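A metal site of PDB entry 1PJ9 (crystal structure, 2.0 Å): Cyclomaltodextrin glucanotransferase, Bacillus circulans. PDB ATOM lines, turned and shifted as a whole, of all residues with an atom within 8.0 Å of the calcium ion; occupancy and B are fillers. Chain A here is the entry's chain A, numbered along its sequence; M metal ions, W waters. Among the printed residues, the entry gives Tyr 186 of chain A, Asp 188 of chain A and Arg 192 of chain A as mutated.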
ATOM      1  N   PRO A 138       0.067  27.064  34.955  1.00  0.00           N
ATOM      2  CA  PRO A 138      -0.135  25.707  34.447  1.00  0.00           C
ATOM      3  C   PRO A 138      -0.903  25.612  33.129  1.00  0.00           C
ATOM      4  O   PRO A 138      -1.289  24.519  32.713  1.00  0.00           O
ATOM      5  CB  PRO A 138      -0.886  25.032  35.598  1.00  0.00           C
ATOM      6  CG  PRO A 138      -1.778  26.148  36.067  1.00  0.00           C
ATOM      7  CD  PRO A 138      -0.856  27.348  36.074  1.00  0.00           C
ATOM      8  N   ASN A 139      -1.126  26.734  32.465  1.00  0.00           N
ATOM      9  CA  ASN A 139      -1.841  26.718  31.194  1.00  0.00           C
ATOM     10  C   ASN A 139      -0.939  26.235  30.062  1.00  0.00           C
ATOM     11  O   ASN A 139      -1.413  25.623  29.104  1.00  0.00           O
ATOM     12  CB  ASN A 139      -2.362  28.113  30.829  1.00  0.00           C
ATOM     13  CG  ASN A 139      -2.978  28.170  29.440  1.00  0.00           C
ATOM     14  OD1 ASN A 139      -4.042  27.583  29.193  1.00  0.00           O
ATOM     15  ND2 ASN A 139      -2.313  28.847  28.521  1.00  0.00           N
ATOM     16  N   HIS A 140       0.351  26.514  30.183  1.00  0.00           N
ATOM     17  CA  HIS A 140       1.291  26.210  29.105  1.00  0.00           C
ATOM     18  C   HIS A 140       2.702  26.017  29.613  1.00  0.00           C
ATOM     19  O   HIS A 140       2.996  26.228  30.792  1.00  0.00           O
ATOM     20  CB  HIS A 140       1.313  27.381  28.130  1.00  0.00           C
ATOM     21  CG  HIS A 140       1.588  28.685  28.810  1.00  0.00           C
ATOM     22  ND1 HIS A 140       0.597  29.456  29.377  1.00  0.00           N
ATOM     23  CD2 HIS A 140       2.762  29.292  29.118  1.00  0.00           C
ATOM     24  CE1 HIS A 140       1.133  30.486  30.002  1.00  0.00           C
ATOM     25  NE2 HIS A 140       2.452  30.408  29.860  1.00  0.00           N
ATOM     26  N   HIS A 176      -2.273  20.596  23.456  1.00  0.00           N
ATOM     27  CA  HIS A 176      -3.367  20.747  22.507  1.00  0.00           C
ATOM     28  C   HIS A 176      -2.789  21.072  21.138  1.00  0.00           C
ATOM     29  O   HIS A 176      -1.792  21.796  21.029  1.00  0.00           O
ATOM     30  CB  HIS A 176      -4.298  21.895  22.936  1.00  0.00           C
ATOM     31  CG  HIS A 176      -5.239  21.526  24.040  1.00  0.00           C
ATOM     32  ND1 HIS A 176      -5.616  22.417  25.029  1.00  0.00           N
ATOM     33  CD2 HIS A 176      -5.932  20.385  24.292  1.00  0.00           C
ATOM     34  CE1 HIS A 176      -6.483  21.846  25.832  1.00  0.00           C
ATOM     35  NE2 HIS A 176      -6.693  20.611  25.403  1.00  0.00           N
ATOM     36  N   TYR A 186     -14.881  31.704  25.002  1.00  0.00           N
ATOM     37  CA  TYR A 186     -14.124  31.111  26.099  1.00  0.00           C
ATOM     38  C   TYR A 186     -13.555  29.757  25.690  1.00  0.00           C
ATOM     39  O   TYR A 186     -12.386  29.459  25.941  1.00  0.00           O
ATOM     40  CB  TYR A 186     -15.005  30.965  27.343  1.00  0.00           C
ATOM     41  CG  TYR A 186     -15.318  32.306  27.955  1.00  0.00           C
ATOM     42  CD1 TYR A 186     -16.599  32.854  27.881  1.00  0.00           C
ATOM     43  CD2 TYR A 186     -14.311  33.062  28.563  1.00  0.00           C
ATOM     44  CE1 TYR A 186     -16.866  34.130  28.388  1.00  0.00           C
ATOM     45  CE2 TYR A 186     -14.564  34.321  29.061  1.00  0.00           C
ATOM     46  CZ  TYR A 186     -15.832  34.860  28.972  1.00  0.00           C
ATOM     47  OH  TYR A 186     -16.063  36.124  29.458  1.00  0.00           O
ATOM     48  N   GLU A 187     -14.384  28.953  25.033  1.00  0.00           N
ATOM     49  CA  GLU A 187     -13.944  27.640  24.567  1.00  0.00           C
ATOM     50  C   GLU A 187     -12.731  27.768  23.643  1.00  0.00           C
ATOM     51  O   GLU A 187     -11.763  27.009  23.763  1.00  0.00           O
ATOM     52  CB  GLU A 187     -15.106  26.955  23.840  1.00  0.00           C
ATOM     53  CG  GLU A 187     -14.706  25.818  22.928  1.00  0.00           C
ATOM     54  CD  GLU A 187     -15.892  25.094  22.328  1.00  0.00           C
ATOM     55  OE1 GLU A 187     -16.988  25.686  22.272  1.00  0.00           O
ATOM     56  OE2 GLU A 187     -15.716  23.939  21.905  1.00  0.00           O
ATOM     57  N   ASP A 188     -12.782  28.738  22.730  1.00  0.00           N
ATOM     58  CA  ASP A 188     -11.699  28.943  21.787  1.00  0.00           C
ATOM     59  C   ASP A 188     -10.402  29.331  22.504  1.00  0.00           C
ATOM     60  O   ASP A 188      -9.322  28.842  22.167  1.00  0.00           O
ATOM     61  CB  ASP A 188     -12.076  30.018  20.766  1.00  0.00           C
ATOM     62  CG  ASP A 188     -11.112  30.083  19.593  1.00  0.00           C
ATOM     63  OD1 ASP A 188     -10.037  30.709  19.733  1.00  0.00           O
ATOM     64  OD2 ASP A 188     -11.422  29.490  18.542  1.00  0.00           O
ATOM     65  N   GLY A 189     -10.521  30.208  23.491  1.00  0.00           N
ATOM     66  CA  GLY A 189      -9.347  30.650  24.229  1.00  0.00           C
ATOM     67  C   GLY A 189      -8.833  29.631  25.236  1.00  0.00           C
ATOM     68  O   GLY A 189      -7.758  29.798  25.810  1.00  0.00           O
ATOM     69  N   ILE A 190      -9.604  28.571  25.454  1.00  0.00           N
ATOM     70  CA  ILE A 190      -9.222  27.534  26.404  1.00  0.00           C
ATOM     71  C   ILE A 190      -8.533  26.337  25.731  1.00  0.00           C
ATOM     72  O   ILE A 190      -7.505  25.848  26.213  1.00  0.00           O
ATOM     73  CB  ILE A 190     -10.460  27.006  27.188  1.00  0.00           C
ATOM     74  CG1 ILE A 190     -10.961  28.077  28.154  1.00  0.00           C
ATOM     75  CG2 ILE A 190     -10.089  25.733  27.959  1.00  0.00           C
ATOM     76  CD1 ILE A 190     -12.279  27.718  28.836  1.00  0.00           C
ATOM     77  N   TYR A 191      -9.097  25.865  24.627  1.00  0.00           N
ATOM     78  CA  TYR A 191      -8.564  24.674  23.974  1.00  0.00           C
ATOM     79  C   TYR A 191      -7.638  24.885  22.773  1.00  0.00           C
ATOM     80  O   TYR A 191      -7.231  23.927  22.122  1.00  0.00           O
ATOM     81  CB  TYR A 191      -9.740  23.761  23.616  1.00  0.00           C
ATOM     82  CG  TYR A 191     -10.456  23.258  24.848  1.00  0.00           C
ATOM     83  CD1 TYR A 191      -9.907  22.227  25.629  1.00  0.00           C
ATOM     84  CD2 TYR A 191     -11.645  23.840  25.282  1.00  0.00           C
ATOM     85  CE1 TYR A 191     -10.532  21.805  26.795  1.00  0.00           C
ATOM     86  CE2 TYR A 191     -12.273  23.423  26.456  1.00  0.00           C
ATOM     87  CZ  TYR A 191     -11.711  22.407  27.206  1.00  0.00           C
ATOM     88  OH  TYR A 191     -12.325  21.990  28.359  1.00  0.00           O
ATOM     89  N   ARG A 192      -7.304  26.138  22.497  1.00  0.00           N
ATOM     90  CA  ARG A 192      -6.355  26.468  21.443  1.00  0.00           C
ATOM     91  C   ARG A 192      -5.191  27.184  22.126  1.00  0.00           C
ATOM     92  O   ARG A 192      -5.321  27.598  23.281  1.00  0.00           O
ATOM     93  CB  ARG A 192      -7.007  27.372  20.379  1.00  0.00           C
ATOM     94  CG  ARG A 192      -8.197  26.742  19.647  1.00  0.00           C
ATOM     95  CD  ARG A 192      -8.632  27.607  18.467  1.00  0.00           C
ATOM     96  NE  ARG A 192      -9.950  27.233  17.940  1.00  0.00           N
ATOM     97  CZ  ARG A 192     -10.207  26.168  17.187  1.00  0.00           C
ATOM     98  NH1 ARG A 192      -9.230  25.334  16.837  1.00  0.00           N
ATOM     99  NH2 ARG A 192     -11.439  25.940  16.770  1.00  0.00           N
ATOM    100  N   ASN A 193      -4.064  27.323  21.428  1.00  0.00           N
ATOM    101  CA  ASN A 193      -2.897  27.954  22.034  1.00  0.00           C
ATOM    102  C   ASN A 193      -3.041  29.458  22.257  1.00  0.00           C
ATOM    103  O   ASN A 193      -3.602  30.179  21.439  1.00  0.00           O
ATOM    104  CB  ASN A 193      -1.635  27.729  21.187  1.00  0.00           C
ATOM    105  CG  ASN A 193      -1.283  26.268  21.034  1.00  0.00           C
ATOM    106  OD1 ASN A 193      -1.590  25.438  21.894  1.00  0.00           O
ATOM    107  ND2 ASN A 193      -0.611  25.946  19.927  1.00  0.00           N
ATOM    108  N   LEU A 194      -2.510  29.919  23.384  1.00  0.00           N
ATOM    109  CA  LEU A 194      -2.471  31.333  23.696  1.00  0.00           C
ATOM    110  C   LEU A 194      -1.194  31.793  22.988  1.00  0.00           C
ATOM    111  O   LEU A 194      -0.090  31.459  23.427  1.00  0.00           O
ATOM    112  CB  LEU A 194      -2.362  31.559  25.208  1.00  0.00           C
ATOM    113  CG  LEU A 194      -2.287  33.001  25.728  1.00  0.00           C
ATOM    114  CD1 LEU A 194      -3.507  33.792  25.287  1.00  0.00           C
ATOM    115  CD2 LEU A 194      -2.186  32.973  27.254  1.00  0.00           C
ATOM    116  N   LEU A 197       2.348  29.746  22.679  1.00  0.00           N
ATOM    117  CA  LEU A 197       2.638  28.955  23.873  1.00  0.00           C
ATOM    118  C   LEU A 197       2.018  27.565  23.806  1.00  0.00           C
ATOM    119  O   LEU A 197       0.817  27.429  23.567  1.00  0.00           O
ATOM    120  CB  LEU A 197       2.122  29.686  25.123  1.00  0.00           C
ATOM    121  CG  LEU A 197       2.684  31.089  25.362  1.00  0.00           C
ATOM    122  CD1 LEU A 197       1.890  31.798  26.450  1.00  0.00           C
ATOM    123  CD2 LEU A 197       4.162  30.994  25.740  1.00  0.00           C
ATOM    124  N   ALA A 198       2.839  26.537  23.999  1.00  0.00           N
ATOM    125  CA  ALA A 198       2.365  25.155  23.972  1.00  0.00           C
ATOM    126  C   ALA A 198       1.293  24.964  25.030  1.00  0.00           C
ATOM    127  O   ALA A 198       1.582  24.973  26.227  1.00  0.00           O
ATOM    128  CB  ALA A 198       3.528  24.193  24.206  1.00  0.00           C
ATOM    129  N   ASP A 199       0.050  24.760  24.595  1.00  0.00           N
ATOM    130  CA  ASP A 199      -1.078  24.611  25.517  1.00  0.00           C
ATOM    131  C   ASP A 199      -1.150  23.226  26.143  1.00  0.00           C
ATOM    132  O   ASP A 199      -1.343  22.226  25.449  1.00  0.00           O
ATOM    133  CB  ASP A 199      -2.400  24.900  24.801  1.00  0.00           C
ATOM    134  CG  ASP A 199      -3.473  25.434  25.727  1.00  0.00           C
ATOM    135  OD1 ASP A 199      -3.208  26.459  26.399  1.00  0.00           O
ATOM    136  OD2 ASP A 199      -4.563  24.843  25.791  1.00  0.00           O
ATOM    137  N   LEU A 200      -0.994  23.169  27.471  1.00  0.00           N
ATOM    138  CA  LEU A 200      -1.054  21.900  28.184  1.00  0.00           C
ATOM    139  C   LEU A 200      -2.467  21.320  28.139  1.00  0.00           C
ATOM    140  O   LEU A 200      -3.459  22.048  28.214  1.00  0.00           O
ATOM    141  CB  LEU A 200      -0.609  22.107  29.644  1.00  0.00           C
ATOM    142  CG  LEU A 200       0.898  22.281  29.847  1.00  0.00           C
ATOM    143  CD1 LEU A 200       1.192  22.725  31.278  1.00  0.00           C
ATOM    144  CD2 LEU A 200       1.591  20.955  29.546  1.00  0.00           C
ATOM    145  N   ASN A 201      -2.535  19.995  28.005  1.00  0.00           N
ATOM    146  CA  ASN A 201      -3.804  19.270  27.965  1.00  0.00           C
ATOM    147  C   ASN A 201      -4.089  18.673  29.335  1.00  0.00           C
ATOM    148  O   ASN A 201      -3.589  17.594  29.676  1.00  0.00           O
ATOM    149  CB  ASN A 201      -3.722  18.153  26.904  1.00  0.00           C
ATOM    150  CG  ASN A 201      -4.943  17.249  26.916  1.00  0.00           C
ATOM    151  OD1 ASN A 201      -5.968  17.575  27.514  1.00  0.00           O
ATOM    152  ND2 ASN A 201      -4.835  16.104  26.252  1.00  0.00           N
ATOM    153  N   HIS A 202      -4.908  19.367  30.124  1.00  0.00           N
ATOM    154  CA  HIS A 202      -5.210  18.911  31.473  1.00  0.00           C
ATOM    155  C   HIS A 202      -6.103  17.667  31.524  1.00  0.00           C
ATOM    156  O   HIS A 202      -6.342  17.125  32.605  1.00  0.00           O
ATOM    157  CB  HIS A 202      -5.820  20.047  32.287  1.00  0.00           C
ATOM    158  CG  HIS A 202      -4.949  21.264  32.344  1.00  0.00           C
ATOM    159  ND1 HIS A 202      -5.074  22.304  31.453  1.00  0.00           N
ATOM    160  CD2 HIS A 202      -3.894  21.566  33.130  1.00  0.00           C
ATOM    161  CE1 HIS A 202      -4.132  23.196  31.684  1.00  0.00           C
ATOM    162  NE2 HIS A 202      -3.397  22.771  32.694  1.00  0.00           N
ATOM    163  N   ALA A 230      -3.447  33.174  33.627  1.00  0.00           N
ATOM    164  CA  ALA A 230      -4.377  32.894  32.532  1.00  0.00           C
ATOM    165  C   ALA A 230      -5.487  31.893  32.848  1.00  0.00           C
ATOM    166  O   ALA A 230      -5.697  30.933  32.089  1.00  0.00           O
ATOM    167  CB  ALA A 230      -3.586  32.415  31.322  1.00  0.00           C
ATOM    168  N   VAL A 231      -6.231  32.108  33.922  1.00  0.00           N
ATOM    169  CA  VAL A 231      -7.285  31.166  34.287  1.00  0.00           C
ATOM    170  C   VAL A 231      -8.459  31.174  33.326  1.00  0.00           C
ATOM    171  O   VAL A 231      -9.253  30.242  33.301  1.00  0.00           O
ATOM    172  CB  VAL A 231      -7.782  31.412  35.726  1.00  0.00           C
ATOM    173  CG1 VAL A 231      -6.624  31.213  36.707  1.00  0.00           C
ATOM    174  CG2 VAL A 231      -8.346  32.820  35.849  1.00  0.00           C
ATOM    175  N   LYS A 232      -8.570  32.234  32.522  1.00  0.00           N
ATOM    176  CA  LYS A 232      -9.640  32.325  31.534  1.00  0.00           C
ATOM    177  C   LYS A 232      -9.331  31.371  30.376  1.00  0.00           C
ATOM    178  O   LYS A 232     -10.186  31.084  29.544  1.00  0.00           O
ATOM    179  CB  LYS A 232      -9.746  33.764  31.023  1.00  0.00           C
ATOM    180  CG  LYS A 232     -10.809  33.977  29.947  1.00  0.00           C
ATOM    181  CD  LYS A 232     -11.047  35.457  29.657  1.00  0.00           C
ATOM    182  CE  LYS A 232      -9.792  36.149  29.147  1.00  0.00           C
ATOM    183  NZ  LYS A 232     -10.059  37.585  28.829  1.00  0.00           N
ATOM    184  N   HIS A 233      -8.101  30.863  30.351  1.00  0.00           N
ATOM    185  CA  HIS A 233      -7.642  29.991  29.274  1.00  0.00           C
ATOM    186  C   HIS A 233      -7.465  28.520  29.617  1.00  0.00           C
ATOM    187  O   HIS A 233      -6.893  27.759  28.834  1.00  0.00           O
ATOM    188  CB  HIS A 233      -6.349  30.559  28.695  1.00  0.00           C
ATOM    189  CG  HIS A 233      -6.496  31.953  28.155  1.00  0.00           C
ATOM    190  ND1 HIS A 233      -7.176  32.222  26.990  1.00  0.00           N
ATOM    191  CD2 HIS A 233      -6.107  33.146  28.654  1.00  0.00           C
ATOM    192  CE1 HIS A 233      -7.196  33.524  26.780  1.00  0.00           C
ATOM    193  NE2 HIS A 233      -6.561  34.111  27.780  1.00  0.00           N
ATOM    194  N   MET A 234      -7.952  28.120  30.789  1.00  0.00           N
ATOM    195  CA  MET A 234      -7.888  26.715  31.208  1.00  0.00           C
ATOM    196  C   MET A 234      -9.301  26.262  31.528  1.00  0.00           C
ATOM    197  O   MET A 234     -10.163  27.082  31.867  1.00  0.00           O
ATOM    198  CB  MET A 234      -6.989  26.558  32.438  1.00  0.00           C
ATOM    199  CG  MET A 234      -5.517  26.842  32.166  1.00  0.00           C
ATOM    200  SD  MET A 234      -4.457  26.552  33.603  1.00  0.00           S
ATOM    201  CE  MET A 234      -4.663  28.098  34.473  1.00  0.00           C
ATOM    202  N   PRO A 235      -9.589  24.953  31.416  1.00  0.00           N
ATOM    203  CA  PRO A 235     -10.929  24.438  31.709  1.00  0.00           C
ATOM    204  C   PRO A 235     -11.320  24.823  33.134  1.00  0.00           C
ATOM    205  O   PRO A 235     -10.601  24.512  34.081  1.00  0.00           O
ATOM    206  CB  PRO A 235     -10.772  22.933  31.538  1.00  0.00           C
ATOM    207  CG  PRO A 235      -9.664  22.812  30.529  1.00  0.00           C
ATOM    208  CD  PRO A 235      -8.689  23.854  31.010  1.00  0.00           C
HETATM  209 CA    CA M   1      -5.338  26.384  27.600  1.00  0.00          CA
HETATM  210  O   HOH W   1      -6.757  24.625  28.369  1.00  0.00           O
HETATM  211  O   HOH W   2      -5.522  28.233  25.993  1.00  0.00           O
HETATM  212  O   HOH W   3      -3.883  24.875  28.852  1.00  0.00           O
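Of the 25 residues printed, 4 come within 4 Å of the calcium ion. The nearest printed residue that does not touch the calcium ion is Met 234 (4.4 Å).
OD1 of Asn 139 binds the calcium ion (2.4 Å). Water W1 is bound to the calcium ion (2.4 Å). The calcium ion is bound by the backbone carbonyl oxygen (O) of His 233. The calcium ion is bound by water W3, at 2.4 Å. The calcium ion is bound by OD1 of Asp 199 (2.4 Å). Water W2 is bound to the calcium ion (2.5 Å). OD2 of Asp 199 binds the calcium ion (2.5 Å). The calcium ion is bound by O of Ile 190, at 2.6 Å. The calcium ion has eight donor atoms within binding distance.
ND1 of His 140 sits at hydrogen-bond distance from ND2 of Asn 139, 3.1 Å away. The side-chain sulfur of Met 234 is in hydrogen-bond range of the backbone NH of Asn 139 (3.5 Å). The backbone NH (N) of Leu 200 is in hydrogen-bond range of the backbone carbonyl oxygen (O) of Asn 139 (3.0 Å). The backbone carbonyl oxygen (O) of Asp 199 sits at hydrogen-bond distance from the backbone NH (N) of His 176 (2.7 Å). The backbone NH of Asp 199 sits close to the side-chain amide oxygen of Asn 193 (3.2 Å). A ring nitrogen (ND1) of His 233 is in hydrogen-bond range of the backbone carbonyl oxygen of Gly 189, 2.8 Å away.
Water W3 bridges O of Asn 139 (2.6 Å) and O of Leu 200 (2.9 Å).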
